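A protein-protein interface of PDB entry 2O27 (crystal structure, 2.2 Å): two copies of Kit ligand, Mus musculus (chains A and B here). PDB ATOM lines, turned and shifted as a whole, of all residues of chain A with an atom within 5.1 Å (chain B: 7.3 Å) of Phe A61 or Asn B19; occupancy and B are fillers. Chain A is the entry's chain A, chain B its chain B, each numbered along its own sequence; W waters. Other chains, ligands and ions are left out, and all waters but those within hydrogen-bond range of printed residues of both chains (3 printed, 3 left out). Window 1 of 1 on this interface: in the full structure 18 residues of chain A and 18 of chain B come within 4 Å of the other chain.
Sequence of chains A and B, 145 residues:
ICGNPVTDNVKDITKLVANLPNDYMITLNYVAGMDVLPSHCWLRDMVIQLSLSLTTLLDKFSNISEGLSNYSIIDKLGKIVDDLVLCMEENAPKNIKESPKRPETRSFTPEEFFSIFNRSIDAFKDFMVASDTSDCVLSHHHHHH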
ATOM      1  N   ASN A  19      14.182 -19.624 -32.533  1.00  0.00           N
ATOM      2  CA  ASN A  19      14.296 -20.661 -31.529  1.00  0.00           C
ATOM      3  C   ASN A  19      13.601 -21.968 -31.925  1.00  0.00           C
ATOM      4  O   ASN A  19      13.455 -22.852 -31.096  1.00  0.00           O
ATOM      5  CB  ASN A  19      13.735 -20.158 -30.205  1.00  0.00           C
ATOM      6  CG  ASN A  19      14.625 -20.497 -29.039  1.00  0.00           C
ATOM      7  OD1 ASN A  19      15.834 -20.559 -29.175  1.00  0.00           O
ATOM      8  ND2 ASN A  19      14.028 -20.711 -27.883  1.00  0.00           N
ATOM      9  N   LEU A  20      13.144 -22.048 -33.174  1.00  0.00           N
ATOM     10  CA  LEU A  20      12.510 -23.238 -33.735  1.00  0.00           C
ATOM     11  C   LEU A  20      13.492 -23.788 -34.755  1.00  0.00           C
ATOM     12  O   LEU A  20      14.194 -23.026 -35.399  1.00  0.00           O
ATOM     13  CB  LEU A  20      11.198 -22.884 -34.437  1.00  0.00           C
ATOM     14  CG  LEU A  20       9.978 -22.747 -33.513  1.00  0.00           C
ATOM     15  CD1 LEU A  20       8.737 -22.378 -34.315  1.00  0.00           C
ATOM     16  CD2 LEU A  20       9.790 -24.097 -32.761  1.00  0.00           C
ATOM     17  N   LEU A  57       0.909 -27.348 -32.587  1.00  0.00           N
ATOM     18  CA  LEU A  57       2.282 -26.906 -32.329  1.00  0.00           C
ATOM     19  C   LEU A  57       2.568 -26.767 -30.829  1.00  0.00           C
ATOM     20  O   LEU A  57       3.595 -27.244 -30.342  1.00  0.00           O
ATOM     21  CB  LEU A  57       2.561 -25.547 -32.988  1.00  0.00           C
ATOM     22  CG  LEU A  57       3.839 -25.247 -33.793  1.00  0.00           C
ATOM     23  CD1 LEU A  57       4.256 -23.795 -33.484  1.00  0.00           C
ATOM     24  CD2 LEU A  57       4.986 -26.217 -33.494  1.00  0.00           C
ATOM     25  N   LEU A  58       1.662 -26.095 -30.116  1.00  0.00           N
ATOM     26  CA  LEU A  58       1.811 -25.865 -28.681  1.00  0.00           C
ATOM     27  C   LEU A  58       2.040 -27.149 -27.872  1.00  0.00           C
ATOM     28  O   LEU A  58       2.879 -27.192 -26.978  1.00  0.00           O
ATOM     29  CB  LEU A  58       0.578 -25.146 -28.118  1.00  0.00           C
ATOM     30  CG  LEU A  58       0.717 -24.779 -26.626  1.00  0.00           C
ATOM     31  CD1 LEU A  58       1.773 -23.699 -26.469  1.00  0.00           C
ATOM     32  CD2 LEU A  58      -0.630 -24.295 -26.066  1.00  0.00           C
ATOM     33  N   ASP A  59       1.283 -28.182 -28.200  1.00  0.00           N
ATOM     34  CA  ASP A  59       1.374 -29.460 -27.515  1.00  0.00           C
ATOM     35  C   ASP A  59       2.747 -30.119 -27.709  1.00  0.00           C
ATOM     36  O   ASP A  59       3.030 -31.170 -27.137  1.00  0.00           O
ATOM     37  CB  ASP A  59       0.254 -30.359 -28.027  1.00  0.00           C
ATOM     38  CG  ASP A  59       0.367 -31.786 -27.528  1.00  0.00           C
ATOM     39  OD1 ASP A  59       0.709 -32.674 -28.330  1.00  0.00           O
ATOM     40  OD2 ASP A  59       0.110 -32.015 -26.333  1.00  0.00           O
ATOM     41  N   LYS A  60       3.611 -29.488 -28.498  1.00  0.00           N
ATOM     42  CA  LYS A  60       4.922 -30.065 -28.717  1.00  0.00           C
ATOM     43  C   LYS A  60       5.975 -29.498 -27.770  1.00  0.00           C
ATOM     44  O   LYS A  60       7.097 -29.945 -27.770  1.00  0.00           O
ATOM     45  CB  LYS A  60       5.354 -29.886 -30.177  1.00  0.00           C
ATOM     46  CG  LYS A  60       4.805 -30.966 -31.116  1.00  0.00           C
ATOM     47  CD  LYS A  60       3.297 -30.924 -31.242  1.00  0.00           C
ATOM     48  CE  LYS A  60       2.702 -32.274 -31.696  1.00  0.00           C
ATOM     49  NZ  LYS A  60       3.397 -32.827 -32.868  1.00  0.00           N
ATOM     50  N   PHE A  61       5.602 -28.524 -26.953  1.00  0.00           N
ATOM     51  CA  PHE A  61       6.559 -27.908 -26.056  1.00  0.00           C
ATOM     52  C   PHE A  61       6.117 -27.967 -24.613  1.00  0.00           C
ATOM     53  O   PHE A  61       4.937 -28.181 -24.340  1.00  0.00           O
ATOM     54  CB  PHE A  61       6.775 -26.435 -26.436  1.00  0.00           C
ATOM     55  CG  PHE A  61       7.273 -26.241 -27.843  1.00  0.00           C
ATOM     56  CD1 PHE A  61       6.388 -26.263 -28.923  1.00  0.00           C
ATOM     57  CD2 PHE A  61       8.629 -26.110 -28.103  1.00  0.00           C
ATOM     58  CE1 PHE A  61       6.857 -26.161 -30.218  1.00  0.00           C
ATOM     59  CE2 PHE A  61       9.102 -26.007 -29.418  1.00  0.00           C
ATOM     60  CZ  PHE A  61       8.204 -26.036 -30.461  1.00  0.00           C
ATOM     61  N   SER A  62       7.069 -27.761 -23.700  1.00  0.00           N
ATOM     62  CA  SER A  62       6.779 -27.738 -22.275  1.00  0.00           C
ATOM     63  C   SER A  62       6.726 -26.271 -21.883  1.00  0.00           C
ATOM     64  O   SER A  62       7.412 -25.431 -22.464  1.00  0.00           O
ATOM     65  CB  SER A  62       7.876 -28.447 -21.458  1.00  0.00           C
ATOM     66  OG  SER A  62       7.868 -29.842 -21.690  1.00  0.00           O
ATOM     67  N   ASN A  63       5.933 -25.954 -20.880  1.00  0.00           N
ATOM     68  CA  ASN A  63       5.819 -24.574 -20.475  1.00  0.00           C
ATOM     69  C   ASN A  63       6.982 -24.128 -19.605  1.00  0.00           C
ATOM     70  O   ASN A  63       6.960 -24.313 -18.392  1.00  0.00           O
ATOM     71  CB  ASN A  63       4.502 -24.358 -19.740  1.00  0.00           C
ATOM     72  CG  ASN A  63       4.288 -22.913 -19.320  1.00  0.00           C
ATOM     73  OD1 ASN A  63       3.289 -22.601 -18.676  1.00  0.00           O
ATOM     74  ND2 ASN A  63       5.211 -22.031 -19.683  1.00  0.00           N
ATOM     75  N   ILE A  64       7.993 -23.544 -20.242  1.00  0.00           N
ATOM     76  CA  ILE A  64       9.151 -23.016 -19.541  1.00  0.00           C
ATOM     77  C   ILE A  64       8.687 -21.672 -18.987  1.00  0.00           C
ATOM     78  O   ILE A  64       8.209 -20.824 -19.740  1.00  0.00           O
ATOM     79  CB  ILE A  64      10.323 -22.781 -20.504  1.00  0.00           C
ATOM     80  CG1 ILE A  64      10.648 -24.076 -21.250  1.00  0.00           C
ATOM     81  CG2 ILE A  64      11.541 -22.274 -19.732  1.00  0.00           C
ATOM     82  CD1 ILE A  64      11.754 -23.938 -22.273  1.00  0.00           C
ATOM     83  N   SER A  69       9.857 -18.495 -23.445  1.00  0.00           N
ATOM     84  CA  SER A  69       9.894 -19.805 -24.042  1.00  0.00           C
ATOM     85  C   SER A  69       9.012 -19.895 -25.271  1.00  0.00           C
ATOM     86  O   SER A  69       8.145 -19.057 -25.488  1.00  0.00           O
ATOM     87  CB  SER A  69       9.441 -20.839 -23.017  1.00  0.00           C
ATOM     88  OG  SER A  69       8.081 -20.674 -22.672  1.00  0.00           O
ATOM     89  N   ASN A  70       9.238 -20.925 -26.071  1.00  0.00           N
ATOM     90  CA  ASN A  70       8.445 -21.141 -27.256  1.00  0.00           C
ATOM     91  C   ASN A  70       7.004 -21.387 -26.826  1.00  0.00           C
ATOM     92  O   ASN A  70       6.070 -20.884 -27.455  1.00  0.00           O
ATOM     93  CB  ASN A  70       8.994 -22.342 -28.044  1.00  0.00           C
ATOM     94  CG  ASN A  70      10.350 -22.049 -28.673  1.00  0.00           C
ATOM     95  OD1 ASN A  70      10.854 -20.933 -28.575  1.00  0.00           O
ATOM     96  ND2 ASN A  70      10.937 -23.049 -29.325  1.00  0.00           N
ATOM     97  N   TYR A  71       6.827 -22.137 -25.736  1.00  0.00           N
ATOM     98  CA  TYR A  71       5.482 -22.437 -25.255  1.00  0.00           C
ATOM     99  C   TYR A  71       4.697 -21.148 -25.022  1.00  0.00           C
ATOM    100  O   TYR A  71       3.581 -21.006 -25.504  1.00  0.00           O
ATOM    101  CB  TYR A  71       5.507 -23.255 -23.936  1.00  0.00           C
ATOM    102  CG  TYR A  71       4.132 -23.648 -23.437  1.00  0.00           C
ATOM    103  CD1 TYR A  71       3.586 -24.891 -23.754  1.00  0.00           C
ATOM    104  CD2 TYR A  71       3.347 -22.761 -22.700  1.00  0.00           C
ATOM    105  CE1 TYR A  71       2.286 -25.250 -23.353  1.00  0.00           C
ATOM    106  CE2 TYR A  71       2.039 -23.111 -22.294  1.00  0.00           C
ATOM    107  CZ  TYR A  71       1.532 -24.362 -22.631  1.00  0.00           C
ATOM    108  OH  TYR A  71       0.273 -24.747 -22.242  1.00  0.00           O
ATOM    109  N   ILE A  74       3.967 -19.055 -28.401  1.00  0.00           N
ATOM    110  CA  ILE A  74       2.966 -19.760 -29.189  1.00  0.00           C
ATOM    111  C   ILE A  74       1.589 -19.665 -28.522  1.00  0.00           C
ATOM    112  O   ILE A  74       0.560 -19.466 -29.192  1.00  0.00           O
ATOM    113  CB  ILE A  74       3.346 -21.257 -29.337  1.00  0.00           C
ATOM    114  CG1 ILE A  74       4.585 -21.393 -30.222  1.00  0.00           C
ATOM    115  CG2 ILE A  74       2.164 -22.063 -29.889  1.00  0.00           C
ATOM    116  CD1 ILE A  74       5.210 -22.814 -30.216  1.00  0.00           C
ATOM    117  N   ILE B  13      20.077 -28.578 -20.128  1.00  0.00           N
ATOM    118  CA  ILE B  13      19.603 -29.545 -21.097  1.00  0.00           C
ATOM    119  C   ILE B  13      18.079 -29.707 -21.009  1.00  0.00           C
ATOM    120  O   ILE B  13      17.412 -29.812 -22.037  1.00  0.00           O
ATOM    121  CB  ILE B  13      20.323 -30.909 -20.897  1.00  0.00           C
ATOM    122  CG1 ILE B  13      21.801 -30.768 -21.295  1.00  0.00           C
ATOM    123  CG2 ILE B  13      19.672 -31.990 -21.742  1.00  0.00           C
ATOM    124  CD1 ILE B  13      22.640 -32.033 -21.069  1.00  0.00           C
ATOM    125  N   THR B  14      17.549 -29.693 -19.790  1.00  0.00           N
ATOM    126  CA  THR B  14      16.122 -29.836 -19.530  1.00  0.00           C
ATOM    127  C   THR B  14      15.330 -28.708 -20.191  1.00  0.00           C
ATOM    128  O   THR B  14      14.266 -28.940 -20.772  1.00  0.00           O
ATOM    129  CB  THR B  14      15.834 -29.832 -17.991  1.00  0.00           C
ATOM    130  OG1 THR B  14      16.438 -30.987 -17.389  1.00  0.00           O
ATOM    131  CG2 THR B  14      14.327 -29.850 -17.707  1.00  0.00           C
ATOM    132  N   LYS B  15      15.845 -27.491 -20.092  1.00  0.00           N
ATOM    133  CA  LYS B  15      15.192 -26.345 -20.704  1.00  0.00           C
ATOM    134  C   LYS B  15      15.252 -26.453 -22.229  1.00  0.00           C
ATOM    135  O   LYS B  15      14.293 -26.103 -22.909  1.00  0.00           O
ATOM    136  CB  LYS B  15      15.843 -25.041 -20.228  1.00  0.00           C
ATOM    137  CG  LYS B  15      14.983 -24.249 -19.245  1.00  0.00           C
ATOM    138  CD  LYS B  15      15.787 -23.189 -18.489  1.00  0.00           C
ATOM    139  CE  LYS B  15      14.892 -22.050 -17.952  1.00  0.00           C
ATOM    140  NZ  LYS B  15      13.681 -22.502 -17.189  1.00  0.00           N
ATOM    141  N   LEU B  16      16.366 -26.960 -22.756  1.00  0.00           N
ATOM    142  CA  LEU B  16      16.525 -27.132 -24.200  1.00  0.00           C
ATOM    143  C   LEU B  16      15.487 -28.129 -24.676  1.00  0.00           C
ATOM    144  O   LEU B  16      14.798 -27.892 -25.650  1.00  0.00           O
ATOM    145  CB  LEU B  16      17.914 -27.682 -24.549  1.00  0.00           C
ATOM    146  CG  LEU B  16      18.597 -27.389 -25.893  1.00  0.00           C
ATOM    147  CD1 LEU B  16      19.285 -28.653 -26.345  1.00  0.00           C
ATOM    148  CD2 LEU B  16      17.643 -26.888 -26.961  1.00  0.00           C
ATOM    149  N   VAL B  17      15.382 -29.261 -23.986  1.00  0.00           N
ATOM    150  CA  VAL B  17      14.419 -30.267 -24.387  1.00  0.00           C
ATOM    151  C   VAL B  17      13.002 -29.683 -24.333  1.00  0.00           C
ATOM    152  O   VAL B  17      12.186 -29.955 -25.205  1.00  0.00           O
ATOM    153  CB  VAL B  17      14.494 -31.523 -23.484  1.00  0.00           C
ATOM    154  CG1 VAL B  17      13.311 -32.440 -23.769  1.00  0.00           C
ATOM    155  CG2 VAL B  17      15.810 -32.274 -23.743  1.00  0.00           C
ATOM    156  N   ALA B  18      12.727 -28.870 -23.318  1.00  0.00           N
ATOM    157  CA  ALA B  18      11.400 -28.267 -23.156  1.00  0.00           C
ATOM    158  C   ALA B  18      11.133 -27.184 -24.194  1.00  0.00           C
ATOM    159  O   ALA B  18       9.983 -26.781 -24.392  1.00  0.00           O
ATOM    160  CB  ALA B  18      11.261 -27.692 -21.749  1.00  0.00           C
ATOM    161  N   ASN B  19      12.200 -26.736 -24.865  1.00  0.00           N
ATOM    162  CA  ASN B  19      12.078 -25.707 -25.872  1.00  0.00           C
ATOM    163  C   ASN B  19      12.313 -26.210 -27.298  1.00  0.00           C
ATOM    164  O   ASN B  19      12.412 -25.410 -28.220  1.00  0.00           O
ATOM    165  CB  ASN B  19      13.036 -24.564 -25.578  1.00  0.00           C
ATOM    166  CG  ASN B  19      12.422 -23.217 -25.863  1.00  0.00           C
ATOM    167  OD1 ASN B  19      13.115 -22.275 -26.235  1.00  0.00           O
ATOM    168  ND2 ASN B  19      11.125 -23.116 -25.692  1.00  0.00           N
ATOM    169  N   LEU B  20      12.439 -27.527 -27.456  1.00  0.00           N
ATOM    170  CA  LEU B  20      12.612 -28.172 -28.750  1.00  0.00           C
ATOM    171  C   LEU B  20      11.306 -28.913 -28.998  1.00  0.00           C
ATOM    172  O   LEU B  20      10.719 -29.426 -28.064  1.00  0.00           O
ATOM    173  CB  LEU B  20      13.756 -29.188 -28.694  1.00  0.00           C
ATOM    174  CG  LEU B  20      15.187 -28.632 -28.739  1.00  0.00           C
ATOM    175  CD1 LEU B  20      16.207 -29.758 -28.603  1.00  0.00           C
ATOM    176  CD2 LEU B  20      15.357 -27.873 -30.079  1.00  0.00           C
ATOM    177  N   PRO B  21      10.836 -29.000 -30.258  1.00  0.00           N
ATOM    178  CA  PRO B  21       9.564 -29.720 -30.462  1.00  0.00           C
ATOM    179  C   PRO B  21       9.737 -31.199 -30.071  1.00  0.00           C
ATOM    180  O   PRO B  21      10.741 -31.792 -30.444  1.00  0.00           O
ATOM    181  CB  PRO B  21       9.304 -29.571 -31.969  1.00  0.00           C
ATOM    182  CG  PRO B  21      10.250 -28.411 -32.407  1.00  0.00           C
ATOM    183  CD  PRO B  21      11.453 -28.613 -31.536  1.00  0.00           C
ATOM    184  N   ASN B  22       8.788 -31.806 -29.351  1.00  0.00           N
ATOM    185  CA  ASN B  22       8.981 -33.224 -28.986  1.00  0.00           C
ATOM    186  C   ASN B  22       8.831 -34.247 -30.141  1.00  0.00           C
ATOM    187  O   ASN B  22       9.054 -35.441 -29.952  1.00  0.00           O
ATOM    188  CB  ASN B  22       8.087 -33.628 -27.795  1.00  0.00           C
ATOM    189  CG  ASN B  22       6.596 -33.453 -28.073  1.00  0.00           C
ATOM    190  OD1 ASN B  22       6.094 -33.828 -29.130  1.00  0.00           O
ATOM    191  ND2 ASN B  22       5.887 -32.888 -27.116  1.00  0.00           N
ATOM    192  N   ASP B  23       8.485 -33.787 -31.337  1.00  0.00           N
ATOM    193  CA  ASP B  23       8.361 -34.684 -32.484  1.00  0.00           C
ATOM    194  C   ASP B  23       9.434 -34.375 -33.534  1.00  0.00           C
ATOM    195  O   ASP B  23       9.452 -34.940 -34.625  1.00  0.00           O
ATOM    196  CB  ASP B  23       6.947 -34.613 -33.077  1.00  0.00           C
ATOM    197  CG  ASP B  23       6.554 -33.219 -33.494  1.00  0.00           C
ATOM    198  OD1 ASP B  23       7.091 -32.244 -32.923  1.00  0.00           O
ATOM    199  OD2 ASP B  23       5.692 -33.100 -34.391  1.00  0.00           O
ATOM    200  N   PHE B  61      19.243 -23.275 -35.862  1.00  0.00           N
ATOM    201  CA  PHE B  61      18.744 -22.155 -35.086  1.00  0.00           C
ATOM    202  C   PHE B  61      19.529 -20.884 -35.355  1.00  0.00           C
ATOM    203  O   PHE B  61      20.600 -20.929 -35.963  1.00  0.00           O
ATOM    204  CB  PHE B  61      18.825 -22.462 -33.585  1.00  0.00           C
ATOM    205  CG  PHE B  61      18.032 -23.664 -33.178  1.00  0.00           C
ATOM    206  CD1 PHE B  61      18.578 -24.953 -33.281  1.00  0.00           C
ATOM    207  CD2 PHE B  61      16.707 -23.529 -32.784  1.00  0.00           C
ATOM    208  CE1 PHE B  61      17.798 -26.064 -33.003  1.00  0.00           C
ATOM    209  CE2 PHE B  61      15.921 -24.656 -32.501  1.00  0.00           C
ATOM    210  CZ  PHE B  61      16.475 -25.914 -32.616  1.00  0.00           C
ATOM    211  N   ILE B  64      20.013 -16.286 -30.771  1.00  0.00           N
ATOM    212  CA  ILE B  64      19.247 -15.325 -29.995  1.00  0.00           C
ATOM    213  C   ILE B  64      20.214 -15.005 -28.866  1.00  0.00           C
ATOM    214  O   ILE B  64      20.811 -15.914 -28.307  1.00  0.00           O
ATOM    215  CB  ILE B  64      17.976 -15.949 -29.397  1.00  0.00           C
ATOM    216  CG1 ILE B  64      17.137 -16.594 -30.498  1.00  0.00           C
ATOM    217  CG2 ILE B  64      17.175 -14.870 -28.668  1.00  0.00           C
ATOM    218  CD1 ILE B  64      15.878 -17.269 -29.998  1.00  0.00           C
ATOM    219  N   LEU B  68      15.889 -17.320 -23.210  1.00  0.00           N
ATOM    220  CA  LEU B  68      16.070 -18.736 -23.503  1.00  0.00           C
ATOM    221  C   LEU B  68      16.571 -18.858 -24.926  1.00  0.00           C
ATOM    222  O   LEU B  68      15.843 -18.551 -25.874  1.00  0.00           O
ATOM    223  CB  LEU B  68      14.754 -19.500 -23.395  1.00  0.00           C
ATOM    224  CG  LEU B  68      14.207 -19.903 -22.030  1.00  0.00           C
ATOM    225  CD1 LEU B  68      12.741 -20.271 -22.190  1.00  0.00           C
ATOM    226  CD2 LEU B  68      15.013 -21.064 -21.458  1.00  0.00           C
ATOM    227  N   SER B  69      17.813 -19.294 -25.086  1.00  0.00           N
ATOM    228  CA  SER B  69      18.336 -19.450 -26.425  1.00  0.00           C
ATOM    229  C   SER B  69      18.825 -20.857 -26.688  1.00  0.00           C
ATOM    230  O   SER B  69      19.791 -21.313 -26.093  1.00  0.00           O
ATOM    231  CB  SER B  69      19.460 -18.463 -26.685  1.00  0.00           C
ATOM    232  OG  SER B  69      19.859 -18.526 -28.040  1.00  0.00           O
ATOM    233  N   ASN B  70      18.144 -21.545 -27.586  1.00  0.00           N
ATOM    234  CA  ASN B  70      18.534 -22.894 -27.946  1.00  0.00           C
ATOM    235  C   ASN B  70      19.907 -22.892 -28.596  1.00  0.00           C
ATOM    236  O   ASN B  70      20.720 -23.781 -28.347  1.00  0.00           O
ATOM    237  CB  ASN B  70      17.502 -23.496 -28.901  1.00  0.00           C
ATOM    238  CG  ASN B  70      16.208 -23.832 -28.205  1.00  0.00           C
ATOM    239  OD1 ASN B  70      16.105 -23.697 -26.998  1.00  0.00           O
ATOM    240  ND2 ASN B  70      15.214 -24.278 -28.968  1.00  0.00           N
ATOM    241  N   ILE B  73      22.578 -22.714 -25.761  1.00  0.00           N
ATOM    242  CA  ILE B  73      22.742 -23.960 -25.004  1.00  0.00           C
ATOM    243  C   ILE B  73      23.423 -25.055 -25.850  1.00  0.00           C
ATOM    244  O   ILE B  73      24.364 -25.704 -25.406  1.00  0.00           O
ATOM    245  CB  ILE B  73      21.363 -24.473 -24.527  1.00  0.00           C
ATOM    246  CG1 ILE B  73      20.642 -23.388 -23.716  1.00  0.00           C
ATOM    247  CG2 ILE B  73      21.533 -25.717 -23.693  1.00  0.00           C
ATOM    248  CD1 ILE B  73      19.144 -23.714 -23.454  1.00  0.00           C
HETATM  249  O   HOH W   1      18.368 -20.055 -30.337  1.00  0.00           O
HETATM  250  O   HOH W   2      12.610 -25.353 -30.842  1.00  0.00           O
HETATM  251  O   HOH W   3       3.166 -34.738 -27.576  1.00  0.00           O
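ND2 of Asn A19 is in hydrogen-bond range of OD1 of Asn B19, 2.4 Å away.
The side-chain amide nitrogen (ND2) of Asn A19 lies within hydrogen-bond range of the backbone carbonyl oxygen (O) of Leu B68 (3.5 Å).
OD1 of Asn A19 lies within hydrogen-bond range of N of Asn B70, 3.0 Å away.
O of Asp A59 sits at hydrogen-bond distance from ND2 of Asn B22 (3.3 Å).
The backbone carbonyl oxygen of Lys A60 sits at hydrogen-bond distance from the backbone NH of Asn B22, at 3.0 Å.
NZ of Lys A60 is in salt-bridge range of OD2 of Asp B23 (2.8 Å).
O of Ala B18 is in hydrogen-bond range of N of Ser A62, at 3.2 Å.
The side-chain amide nitrogen (ND2) of Asn B19 sits close to the backbone NH (N) of Asn A70, 2.9 Å away.
Of chain B, only Ala B18 (3.8 Å), Asn B19 (3.6 Å), Leu B20 (3.7 Å) and Pro B21 (3.6 Å) come within 4 Å of Phe A61.
Of the printed residues of chain A, Pro B21 touches Lys A60 (3.7 Å) and Phe A61 (3.6 Å).
Of the printed residues of chain A, Asn B22 touches Asp A59 and Lys A60.
Ile B73 touches none of the printed residues of chain A.
The nearest residue of chain B that does not touch Phe A61 is Asn B22 (4.4 Å).
The nearest residue of chain A that does not touch Asn B19 is Tyr A71 (4.4 Å).
CE2 of Phe B61 touches O of Asn A19 (3.4 Å).
CA of Ser B69 touches OD1 of Asn A19, 3.9 Å away.
Lys A60 touches Pro B21.
Leu B20 touches Phe A61.
CE2 of Phe A61 touches N of Pro B21, 3.6 Å away.
NZ of Lys B15 touches CG2 of Ile A64, at 3.3 Å.
Ala B18 touches Ile A64 (CB to CG1, 3.7 Å).
Ile A64 touches Asn B19 (CD1 to ND2, 3.6 Å).
CG2 of Ile A64 touches CD1 of Leu B68, at 3.4 Å.
Ser A69 touches Asn B19.
O of Asn A19 is in hydrogen-bond range of ND2 of Asn A70, 3.1 Å away.
The backbone carbonyl oxygen (O) of Ile A64 lies within hydrogen-bond range of the side-chain hydroxyl (OG) of Ser A69, at 2.9 Å.
O of Asn B19 is in hydrogen-bond range of ND2 of Asn B70, at 3.1 Å.
O of Ile B64 is in hydrogen-bond range of OG of Ser B69, at 2.8 Å.
Water W2 lies within hydrogen-bond range of O of Asn B19, O of Asn A19, ND2 of Asn A70 and ND2 of Asn B70.
Water W1 lies within hydrogen-bond range of the side-chain amide oxygen of Asn A19 (2.8 Å), the side-chain hydroxyl of Ser B69 (3.1 Å) and the backbone NH of Asn B70 (3.1 Å).
Water W3 lies within hydrogen-bond range of OD1 of Asp A59 (3.3 Å) and ND2 of Asn B22 (3.3 Å).
Asn A19 touches its own counterpart, Asn B19.
Asn A19 touches Phe B61, and with the chains exchanged Phe A61 touches Asn B19.
Asn A19 touches Ile B64, and with the chains exchanged Ile A64 touches Asn B19.
Asn A19 touches Ser B69, and with the chains exchanged Ser A69 touches Asn B19.
Of the 24 pairs that touch across the chains among the printed residues, 11 have their exchanged pair printed and touching as well.
Of the 14 printed residues of chain A, 9 touch a printed residue of chain B.
Hydrophobic or aromatic side chains of chain A within 4 Å of the printed part of chain B: Phe A61 and Ile A64.
Hydrophobic or aromatic side chains of chain B within 4 Å of the printed part of chain A: Ala B18, Pro B21, Phe B61, Ile B64 and Leu B68.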
